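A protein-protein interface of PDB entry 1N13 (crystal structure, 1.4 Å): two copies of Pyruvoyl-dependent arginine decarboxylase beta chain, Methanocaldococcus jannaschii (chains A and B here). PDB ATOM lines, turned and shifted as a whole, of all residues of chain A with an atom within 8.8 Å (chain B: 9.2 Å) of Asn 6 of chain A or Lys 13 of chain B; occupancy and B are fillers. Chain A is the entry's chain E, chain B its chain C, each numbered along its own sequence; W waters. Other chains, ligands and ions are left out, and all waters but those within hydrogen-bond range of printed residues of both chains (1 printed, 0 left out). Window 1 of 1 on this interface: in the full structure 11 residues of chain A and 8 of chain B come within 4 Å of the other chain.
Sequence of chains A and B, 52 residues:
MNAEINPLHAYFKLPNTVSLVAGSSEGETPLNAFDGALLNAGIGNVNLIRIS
O of Tyr 11 of chain B sits at hydrogen-bond distance from ND1 of His 9 of chain A (2.6 Å).
The backbone NH (N) of Asn 6 of chain A is in hydrogen-bond range of the backbone carbonyl oxygen (O) of Phe 12 of chain B.
The side-chain carboxylate (OE1) of Glu 4 of chain A is in hydrogen-bond range of the backbone NH (N) of Leu 14 of chain B, at 3.1 Å.
The backbone carbonyl oxygen of Leu 8 of chain B lies within hydrogen-bond range of the side-chain amino group of Lys 13 of chain B.
The backbone carbonyl oxygen (O) of His 9 of chain B is in hydrogen-bond range of the side-chain amino group (NZ) of Lys 13 of chain B, at 3.2 Å.
OD1 of Asn 6 of chain A sits at hydrogen-bond distance from N of Leu 8 of chain A (2.9 Å).
Among the printed residues, pairs that only touch across the chains: Glu 4 of chain A with Phe 12 of chain B, Glu 4 of chain A with Lys 13 of chain B, Ile 5 of chain A with Phe 12 of chain B, Ile 5 of chain A with Leu 14 of chain B, Asn 6 of chain A with Lys 13 of chain B, Leu 8 of chain A with Ile 49 of chain B, His 9 of chain A with Phe 12 of chain B, Ala 10 of chain A with Phe 12 of chain B, Phe 12 of chain A with Phe 12 of chain B and Ile 49 of chain A with Ile 49 of chain B.
Of the printed residues of chain B, Glu 4 of chain A touches Phe 12 (3.9 Å), Lys 13 (3.5 Å) and Leu 14 (3.1 Å).
Ile 5 of chain A touches just these residues of chain B: Phe 12 and Leu 14.
Of chain B, only Phe 12 (2.9 Å) and Lys 13 (3.4 Å) come within 4 Å of Asn 6 of chain A.
No residue of chain B comes within 4 Å of Pro 7 of chain A.
Leu 8 of chain A touches one residue of chain B.
Ala 10 of chain A touches just one residue of chain B: Phe 12 (3.8 Å).
Printed residues of chain A within 4 Å of Tyr 11 of chain B: His 9.
Of chain A, only Glu 4 (3.5 Å) and Asn 6 (3.4 Å) come within 4 Å of Lys 13 of chain B.
The nearest residue of chain B that does not touch Asn 6 of chain A is Tyr 11 of chain B (4.2 Å).
Printed residues of chain B that touch a printed residue of chain A: Tyr 11, Phe 12, Lys 13, Leu 14 and Ile 49.
Along chain B the printed residues that touch a printed residue of chain A span positions 11 to 49.
Of the 12 printed residues of chain A, 8 touch a printed residue of chain B.
Hydrophobic or aromatic side chains of chain A that line the printed part of chain B: Leu 8, His 9, Ala 10, Phe 12 and Ile 49.
Among the printed residues, 13 pairs touch across the chains.
Among the printed residues, no Asp or Glu carboxylate lies within 4 Å of a Lys or Arg side-chain nitrogen of the other chain.
Leu 8 of chain A touches Ile 49 of chain B, but with the chains exchanged Ile 49 of chain A does not touch Leu 8 of chain B (18.7 Å).
His 9 of chain A touches Tyr 11 of chain B, but with the chains exchanged Tyr 11 of chain A does not touch His 9 of chain B (11.1 Å).
Phe 12 of chain B touches its own counterpart, Phe 12 of chain A.
Ile 49 of chain B touches its own counterpart, Ile 49 of chain A.
Positions printed for both chains: 6, 7, 8, 9, 10, 11, 12, 13 and 49.
Of the 13 pairs that touch across the chains among the printed residues, 2 have their exchanged pair printed and touching as well.
Water W1 lies within hydrogen-bond range of O of Leu 14 of chain B and OE1 of Glu 4 of chain A.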
ATOM      1  N   ALA A   3      17.310  10.867 -14.469  1.00  0.00           N
ATOM      2  CA  ALA A   3      18.547  10.300 -15.088  1.00  0.00           C
ATOM      3  C   ALA A   3      19.681  10.196 -14.071  1.00  0.00           C
ATOM      4  O   ALA A   3      20.747   9.651 -14.365  1.00  0.00           O
ATOM      5  CB  ALA A   3      18.976  11.154 -16.266  1.00  0.00           C
ATOM      6  N   GLU A   4      19.441  10.711 -12.871  1.00  0.00           N
ATOM      7  CA  GLU A   4      20.437  10.677 -11.808  1.00  0.00           C
ATOM      8  C   GLU A   4      20.508   9.319 -11.127  1.00  0.00           C
ATOM      9  O   GLU A   4      19.532   8.564 -11.112  1.00  0.00           O
ATOM     10  CB  GLU A   4      20.132  11.744 -10.762  1.00  0.00           C
ATOM     11  CG  GLU A   4      20.137  13.156 -11.302  1.00  0.00           C
ATOM     12  CD  GLU A   4      19.845  14.190 -10.234  1.00  0.00           C
ATOM     13  OE1 GLU A   4      19.472  13.804  -9.103  1.00  0.00           O
ATOM     14  OE2 GLU A   4      19.991  15.394 -10.528  1.00  0.00           O
ATOM     15  N   ILE A   5      21.670   9.019 -10.559  1.00  0.00           N
ATOM     16  CA  ILE A   5      21.864   7.762  -9.854  1.00  0.00           C
ATOM     17  C   ILE A   5      22.909   7.861  -8.749  1.00  0.00           C
ATOM     18  O   ILE A   5      23.949   8.498  -8.918  1.00  0.00           O
ATOM     19  CB  ILE A   5      22.276   6.612 -10.814  1.00  0.00           C
ATOM     20  CG1 ILE A   5      22.411   5.303 -10.027  1.00  0.00           C
ATOM     21  CG2 ILE A   5      23.594   6.948 -11.529  1.00  0.00           C
ATOM     22  CD1 ILE A   5      22.703   4.096 -10.874  1.00  0.00           C
ATOM     23  N   ASN A   6      22.574   7.319  -7.583  1.00  0.00           N
ATOM     24  CA  ASN A   6      23.520   7.270  -6.476  1.00  0.00           C
ATOM     25  C   ASN A   6      23.897   5.792  -6.425  1.00  0.00           C
ATOM     26  O   ASN A   6      23.108   4.965  -5.973  1.00  0.00           O
ATOM     27  CB  ASN A   6      22.884   7.690  -5.143  1.00  0.00           C
ATOM     28  CG  ASN A   6      23.865   7.595  -3.982  1.00  0.00           C
ATOM     29  OD1 ASN A   6      24.904   6.942  -4.092  1.00  0.00           O
ATOM     30  ND2 ASN A   6      23.555   8.260  -2.876  1.00  0.00           N
ATOM     31  N   PRO A   7      25.096   5.439  -6.922  1.00  0.00           N
ATOM     32  CA  PRO A   7      25.592   4.056  -6.948  1.00  0.00           C
ATOM     33  C   PRO A   7      25.707   3.395  -5.570  1.00  0.00           C
ATOM     34  O   PRO A   7      25.773   2.170  -5.471  1.00  0.00           O
ATOM     35  CB  PRO A   7      26.965   4.200  -7.612  1.00  0.00           C
ATOM     36  CG  PRO A   7      26.818   5.414  -8.464  1.00  0.00           C
ATOM     37  CD  PRO A   7      26.073   6.347  -7.547  1.00  0.00           C
ATOM     38  N   LEU A   8      25.751   4.213  -4.521  1.00  0.00           N
ATOM     39  CA  LEU A   8      25.845   3.728  -3.144  1.00  0.00           C
ATOM     40  C   LEU A   8      24.483   3.263  -2.629  1.00  0.00           C
ATOM     41  O   LEU A   8      24.402   2.556  -1.623  1.00  0.00           O
ATOM     42  CB  LEU A   8      26.376   4.824  -2.218  1.00  0.00           C
ATOM     43  CG  LEU A   8      27.737   5.439  -2.539  1.00  0.00           C
ATOM     44  CD1 LEU A   8      28.006   6.580  -1.575  1.00  0.00           C
ATOM     45  CD2 LEU A   8      28.828   4.385  -2.451  1.00  0.00           C
ATOM     46  N   HIS A   9      23.415   3.728  -3.274  1.00  0.00           N
ATOM     47  CA  HIS A   9      22.063   3.334  -2.888  1.00  0.00           C
ATOM     48  C   HIS A   9      21.476   2.319  -3.866  1.00  0.00           C
ATOM     49  O   HIS A   9      20.807   1.371  -3.456  1.00  0.00           O
ATOM     50  CB  HIS A   9      21.159   4.560  -2.743  1.00  0.00           C
ATOM     51  CG  HIS A   9      21.469   5.391  -1.536  1.00  0.00           C
ATOM     52  ND1 HIS A   9      20.871   6.611  -1.298  1.00  0.00           N
ATOM     53  CD2 HIS A   9      22.291   5.164  -0.484  1.00  0.00           C
ATOM     54  CE1 HIS A   9      21.309   7.096  -0.149  1.00  0.00           C
ATOM     55  NE2 HIS A   9      22.172   6.239   0.365  1.00  0.00           N
ATOM     56  N   ALA A  10      21.739   2.516  -5.155  1.00  0.00           N
ATOM     57  CA  ALA A  10      21.278   1.599  -6.196  1.00  0.00           C
ATOM     58  C   ALA A  10      22.381   0.552  -6.381  1.00  0.00           C
ATOM     59  O   ALA A  10      23.032   0.482  -7.425  1.00  0.00           O
ATOM     60  CB  ALA A  10      21.032   2.358  -7.500  1.00  0.00           C
ATOM     61  N   TYR A  11      22.596  -0.238  -5.332  1.00  0.00           N
ATOM     62  CA  TYR A  11      23.624  -1.276  -5.301  1.00  0.00           C
ATOM     63  C   TYR A  11      23.414  -2.358  -6.359  1.00  0.00           C
ATOM     64  O   TYR A  11      24.340  -3.093  -6.706  1.00  0.00           O
ATOM     65  CB  TYR A  11      23.661  -1.917  -3.907  1.00  0.00           C
ATOM     66  CG  TYR A  11      22.416  -2.713  -3.565  1.00  0.00           C
ATOM     67  CD1 TYR A  11      22.311  -4.061  -3.916  1.00  0.00           C
ATOM     68  CD2 TYR A  11      21.337  -2.118  -2.909  1.00  0.00           C
ATOM     69  CE1 TYR A  11      21.168  -4.791  -3.629  1.00  0.00           C
ATOM     70  CE2 TYR A  11      20.184  -2.844  -2.616  1.00  0.00           C
ATOM     71  CZ  TYR A  11      20.110  -4.179  -2.979  1.00  0.00           C
ATOM     72  OH  TYR A  11      18.982  -4.913  -2.698  1.00  0.00           O
ATOM     73  N   PHE A  12      22.174  -2.461  -6.830  1.00  0.00           N
ATOM     74  CA  PHE A  12      21.764  -3.437  -7.835  1.00  0.00           C
ATOM     75  C   PHE A  12      22.008  -2.981  -9.272  1.00  0.00           C
ATOM     76  O   PHE A  12      21.727  -3.721 -10.217  1.00  0.00           O
ATOM     77  CB  PHE A  12      20.281  -3.767  -7.644  1.00  0.00           C
ATOM     78  CG  PHE A  12      19.419  -2.556  -7.441  1.00  0.00           C
ATOM     79  CD1 PHE A  12      18.942  -1.832  -8.527  1.00  0.00           C
ATOM     80  CD2 PHE A  12      19.106  -2.125  -6.157  1.00  0.00           C
ATOM     81  CE1 PHE A  12      18.165  -0.692  -8.337  1.00  0.00           C
ATOM     82  CE2 PHE A  12      18.331  -0.988  -5.955  1.00  0.00           C
ATOM     83  CZ  PHE A  12      17.860  -0.269  -7.050  1.00  0.00           C
ATOM     84  N   LYS A  13      22.467  -1.746  -9.442  1.00  0.00           N
ATOM     85  CA  LYS A  13      22.751  -1.223 -10.769  1.00  0.00           C
ATOM     86  C   LYS A  13      24.236  -0.893 -10.856  1.00  0.00           C
ATOM     87  O   LYS A  13      24.677   0.167 -10.421  1.00  0.00           O
ATOM     88  CB  LYS A  13      21.893   0.009 -11.067  1.00  0.00           C
ATOM     89  CG  LYS A  13      22.013   0.512 -12.498  1.00  0.00           C
ATOM     90  CD  LYS A  13      20.996   1.606 -12.794  1.00  0.00           C
ATOM     91  CE  LYS A  13      21.203   2.195 -14.183  1.00  0.00           C
ATOM     92  NZ  LYS A  13      21.084   1.177 -15.268  1.00  0.00           N
ATOM     93  N   ILE A  49      34.075   8.987  -5.789  1.00  0.00           N
ATOM     94  CA  ILE A  49      33.930   8.016  -4.713  1.00  0.00           C
ATOM     95  C   ILE A  49      35.065   7.037  -5.003  1.00  0.00           C
ATOM     96  O   ILE A  49      34.990   6.248  -5.949  1.00  0.00           O
ATOM     97  CB  ILE A  49      32.590   7.265  -4.787  1.00  0.00           C
ATOM     98  CG1 ILE A  49      31.427   8.237  -4.578  1.00  0.00           C
ATOM     99  CG2 ILE A  49      32.556   6.146  -3.747  1.00  0.00           C
ATOM    100  CD1 ILE A  49      30.074   7.570  -4.623  1.00  0.00           C
ATOM    101  N   ASN B   6       4.569  14.491  -6.332  1.00  0.00           N
ATOM    102  CA  ASN B   6       5.548  14.161  -5.299  1.00  0.00           C
ATOM    103  C   ASN B   6       6.614  13.206  -5.836  1.00  0.00           C
ATOM    104  O   ASN B   6       6.297  12.136  -6.357  1.00  0.00           O
ATOM    105  CB  ASN B   6       4.846  13.538  -4.085  1.00  0.00           C
ATOM    106  CG  ASN B   6       5.803  13.246  -2.942  1.00  0.00           C
ATOM    107  OD1 ASN B   6       5.799  12.151  -2.376  1.00  0.00           O
ATOM    108  ND2 ASN B   6       6.625  14.230  -2.592  1.00  0.00           N
ATOM    109  N   PRO B   7       7.896  13.594  -5.735  1.00  0.00           N
ATOM    110  CA  PRO B   7       9.001  12.759  -6.217  1.00  0.00           C
ATOM    111  C   PRO B   7       9.145  11.436  -5.465  1.00  0.00           C
ATOM    112  O   PRO B   7       9.053  11.392  -4.236  1.00  0.00           O
ATOM    113  CB  PRO B   7      10.223  13.654  -5.990  1.00  0.00           C
ATOM    114  CG  PRO B   7       9.663  15.036  -6.109  1.00  0.00           C
ATOM    115  CD  PRO B   7       8.389  14.917  -5.316  1.00  0.00           C
ATOM    116  N   LEU B   8       9.331  10.358  -6.223  1.00  0.00           N
ATOM    117  CA  LEU B   8       9.520   9.023  -5.661  1.00  0.00           C
ATOM    118  C   LEU B   8      10.940   8.586  -6.010  1.00  0.00           C
ATOM    119  O   LEU B   8      11.562   9.161  -6.904  1.00  0.00           O
ATOM    120  CB  LEU B   8       8.512   8.034  -6.253  1.00  0.00           C
ATOM    121  CG  LEU B   8       7.028   8.318  -6.007  1.00  0.00           C
ATOM    122  CD1 LEU B   8       6.191   7.350  -6.814  1.00  0.00           C
ATOM    123  CD2 LEU B   8       6.698   8.205  -4.527  1.00  0.00           C
ATOM    124  N   HIS B   9      11.447   7.574  -5.308  1.00  0.00           N
ATOM    125  CA  HIS B   9      12.803   7.068  -5.538  1.00  0.00           C
ATOM    126  C   HIS B   9      13.842   8.176  -5.427  1.00  0.00           C
ATOM    127  O   HIS B   9      14.872   8.147  -6.104  1.00  0.00           O
ATOM    128  CB  HIS B   9      12.913   6.386  -6.904  1.00  0.00           C
ATOM    129  CG  HIS B   9      12.298   5.023  -6.949  1.00  0.00           C
ATOM    130  ND1 HIS B   9      11.752   4.488  -8.095  1.00  0.00           N
ATOM    131  CD2 HIS B   9      12.149   4.082  -5.987  1.00  0.00           C
ATOM    132  CE1 HIS B   9      11.295   3.276  -7.838  1.00  0.00           C
ATOM    133  NE2 HIS B   9      11.524   3.006  -6.565  1.00  0.00           N
ATOM    134  N   ALA B  10      13.560   9.150  -4.565  1.00  0.00           N
ATOM    135  CA  ALA B  10      14.455  10.281  -4.355  1.00  0.00           C
ATOM    136  C   ALA B  10      15.828   9.847  -3.845  1.00  0.00           C
ATOM    137  O   ALA B  10      16.846  10.403  -4.255  1.00  0.00           O
ATOM    138  CB  ALA B  10      13.825  11.278  -3.390  1.00  0.00           C
ATOM    139  N   TYR B  11      15.858   8.833  -2.982  1.00  0.00           N
ATOM    140  CA  TYR B  11      17.124   8.354  -2.429  1.00  0.00           C
ATOM    141  C   TYR B  11      18.032   7.654  -3.435  1.00  0.00           C
ATOM    142  O   TYR B  11      19.211   7.429  -3.159  1.00  0.00           O
ATOM    143  CB  TYR B  11      16.879   7.459  -1.216  1.00  0.00           C
ATOM    144  CG  TYR B  11      16.477   8.231   0.013  1.00  0.00           C
ATOM    145  CD1 TYR B  11      17.425   8.611   0.958  1.00  0.00           C
ATOM    146  CD2 TYR B  11      15.151   8.609   0.219  1.00  0.00           C
ATOM    147  CE1 TYR B  11      17.068   9.348   2.079  1.00  0.00           C
ATOM    148  CE2 TYR B  11      14.781   9.350   1.339  1.00  0.00           C
ATOM    149  CZ  TYR B  11      15.747   9.716   2.262  1.00  0.00           C
ATOM    150  OH  TYR B  11      15.397  10.458   3.365  1.00  0.00           O
ATOM    151  N   PHE B  12      17.490   7.320  -4.603  1.00  0.00           N
ATOM    152  CA  PHE B  12      18.278   6.664  -5.643  1.00  0.00           C
ATOM    153  C   PHE B  12      18.917   7.670  -6.583  1.00  0.00           C
ATOM    154  O   PHE B  12      19.707   7.308  -7.453  1.00  0.00           O
ATOM    155  CB  PHE B  12      17.416   5.677  -6.428  1.00  0.00           C
ATOM    156  CG  PHE B  12      17.054   4.454  -5.649  1.00  0.00           C
ATOM    157  CD1 PHE B  12      18.040   3.569  -5.231  1.00  0.00           C
ATOM    158  CD2 PHE B  12      15.732   4.191  -5.314  1.00  0.00           C
ATOM    159  CE1 PHE B  12      17.716   2.442  -4.492  1.00  0.00           C
ATOM    160  CE2 PHE B  12      15.396   3.065  -4.574  1.00  0.00           C
ATOM    161  CZ  PHE B  12      16.390   2.188  -4.160  1.00  0.00           C
ATOM    162  N   LYS B  13      18.559   8.937  -6.404  1.00  0.00           N
ATOM    163  CA  LYS B  13      19.092  10.015  -7.218  1.00  0.00           C
ATOM    164  C   LYS B  13      20.219  10.717  -6.469  1.00  0.00           C
ATOM    165  O   LYS B  13      20.696  10.216  -5.450  1.00  0.00           O
ATOM    166  CB  LYS B  13      17.978  10.992  -7.582  1.00  0.00           C
ATOM    167  CG  LYS B  13      16.884  10.360  -8.426  1.00  0.00           C
ATOM    168  CD  LYS B  13      15.773  11.345  -8.737  1.00  0.00           C
ATOM    169  CE  LYS B  13      14.667  10.680  -9.549  1.00  0.00           C
ATOM    170  NZ  LYS B  13      14.059   9.524  -8.825  1.00  0.00           N
ATOM    171  N   LEU B  14      20.653  11.862  -6.983  1.00  0.00           N
ATOM    172  CA  LEU B  14      21.740  12.622  -6.368  1.00  0.00           C
ATOM    173  C   LEU B  14      21.308  13.350  -5.098  1.00  0.00           C
ATOM    174  O   LEU B  14      20.160  13.797  -4.985  1.00  0.00           O
ATOM    175  CB  LEU B  14      22.283  13.649  -7.366  1.00  0.00           C
ATOM    176  CG  LEU B  14      23.639  13.412  -8.034  1.00  0.00           C
ATOM    177  CD1 LEU B  14      23.839  11.956  -8.386  1.00  0.00           C
ATOM    178  CD2 LEU B  14      23.762  14.309  -9.258  1.00  0.00           C
ATOM    179  N   PRO B  15      22.212  13.442  -4.103  1.00  0.00           N
ATOM    180  CA  PRO B  15      21.879  14.138  -2.856  1.00  0.00           C
ATOM    181  C   PRO B  15      21.507  15.582  -3.187  1.00  0.00           C
ATOM    182  O   PRO B  15      22.061  16.169  -4.116  1.00  0.00           O
ATOM    183  CB  PRO B  15      23.197  14.088  -2.083  1.00  0.00           C
ATOM    184  CG  PRO B  15      23.779  12.791  -2.510  1.00  0.00           C
ATOM    185  CD  PRO B  15      23.535  12.798  -4.003  1.00  0.00           C
ATOM    186  N   ASN B  16      20.559  16.145  -2.448  1.00  0.00           N
ATOM    187  CA  ASN B  16      20.140  17.516  -2.704  1.00  0.00           C
ATOM    188  C   ASN B  16      20.305  18.471  -1.528  1.00  0.00           C
ATOM    189  O   ASN B  16      19.750  19.566  -1.538  1.00  0.00           O
ATOM    190  CB  ASN B  16      18.704  17.555  -3.237  1.00  0.00           C
ATOM    191  CG  ASN B  16      17.742  16.749  -2.392  1.00  0.00           C
ATOM    192  OD1 ASN B  16      17.923  16.606  -1.186  1.00  0.00           O
ATOM    193  ND2 ASN B  16      16.712  16.209  -3.029  1.00  0.00           N
ATOM    194  N   ILE B  49      31.252   8.066   3.610  1.00  0.00           N
ATOM    195  CA  ILE B  49      31.815   7.634   2.333  1.00  0.00           C
ATOM    196  C   ILE B  49      32.560   8.881   1.870  1.00  0.00           C
ATOM    197  O   ILE B  49      31.952   9.838   1.393  1.00  0.00           O
ATOM    198  CB  ILE B  49      30.723   7.284   1.298  1.00  0.00           C
ATOM    199  CG1 ILE B  49      29.805   6.176   1.828  1.00  0.00           C
ATOM    200  CG2 ILE B  49      31.366   6.868  -0.022  1.00  0.00           C
ATOM    201  CD1 ILE B  49      30.488   4.864   2.046  1.00  0.00           C
ATOM    202  N   ILE B  51      34.175  11.616  -0.104  1.00  0.00           N
ATOM    203  CA  ILE B  51      34.132  12.076  -1.482  1.00  0.00           C
ATOM    204  C   ILE B  51      35.355  12.955  -1.682  1.00  0.00           C
ATOM    205  O   ILE B  51      35.761  13.685  -0.774  1.00  0.00           O
ATOM    206  CB  ILE B  51      32.816  12.837  -1.822  1.00  0.00           C
ATOM    207  CG1 ILE B  51      32.504  13.901  -0.771  1.00  0.00           C
ATOM    208  CG2 ILE B  51      31.661  11.850  -1.940  1.00  0.00           C
ATOM    209  CD1 ILE B  51      31.208  14.653  -1.040  1.00  0.00           C
HETATM  210  O   HOH W   1      18.581  15.050  -6.820  1.00  0.00           O
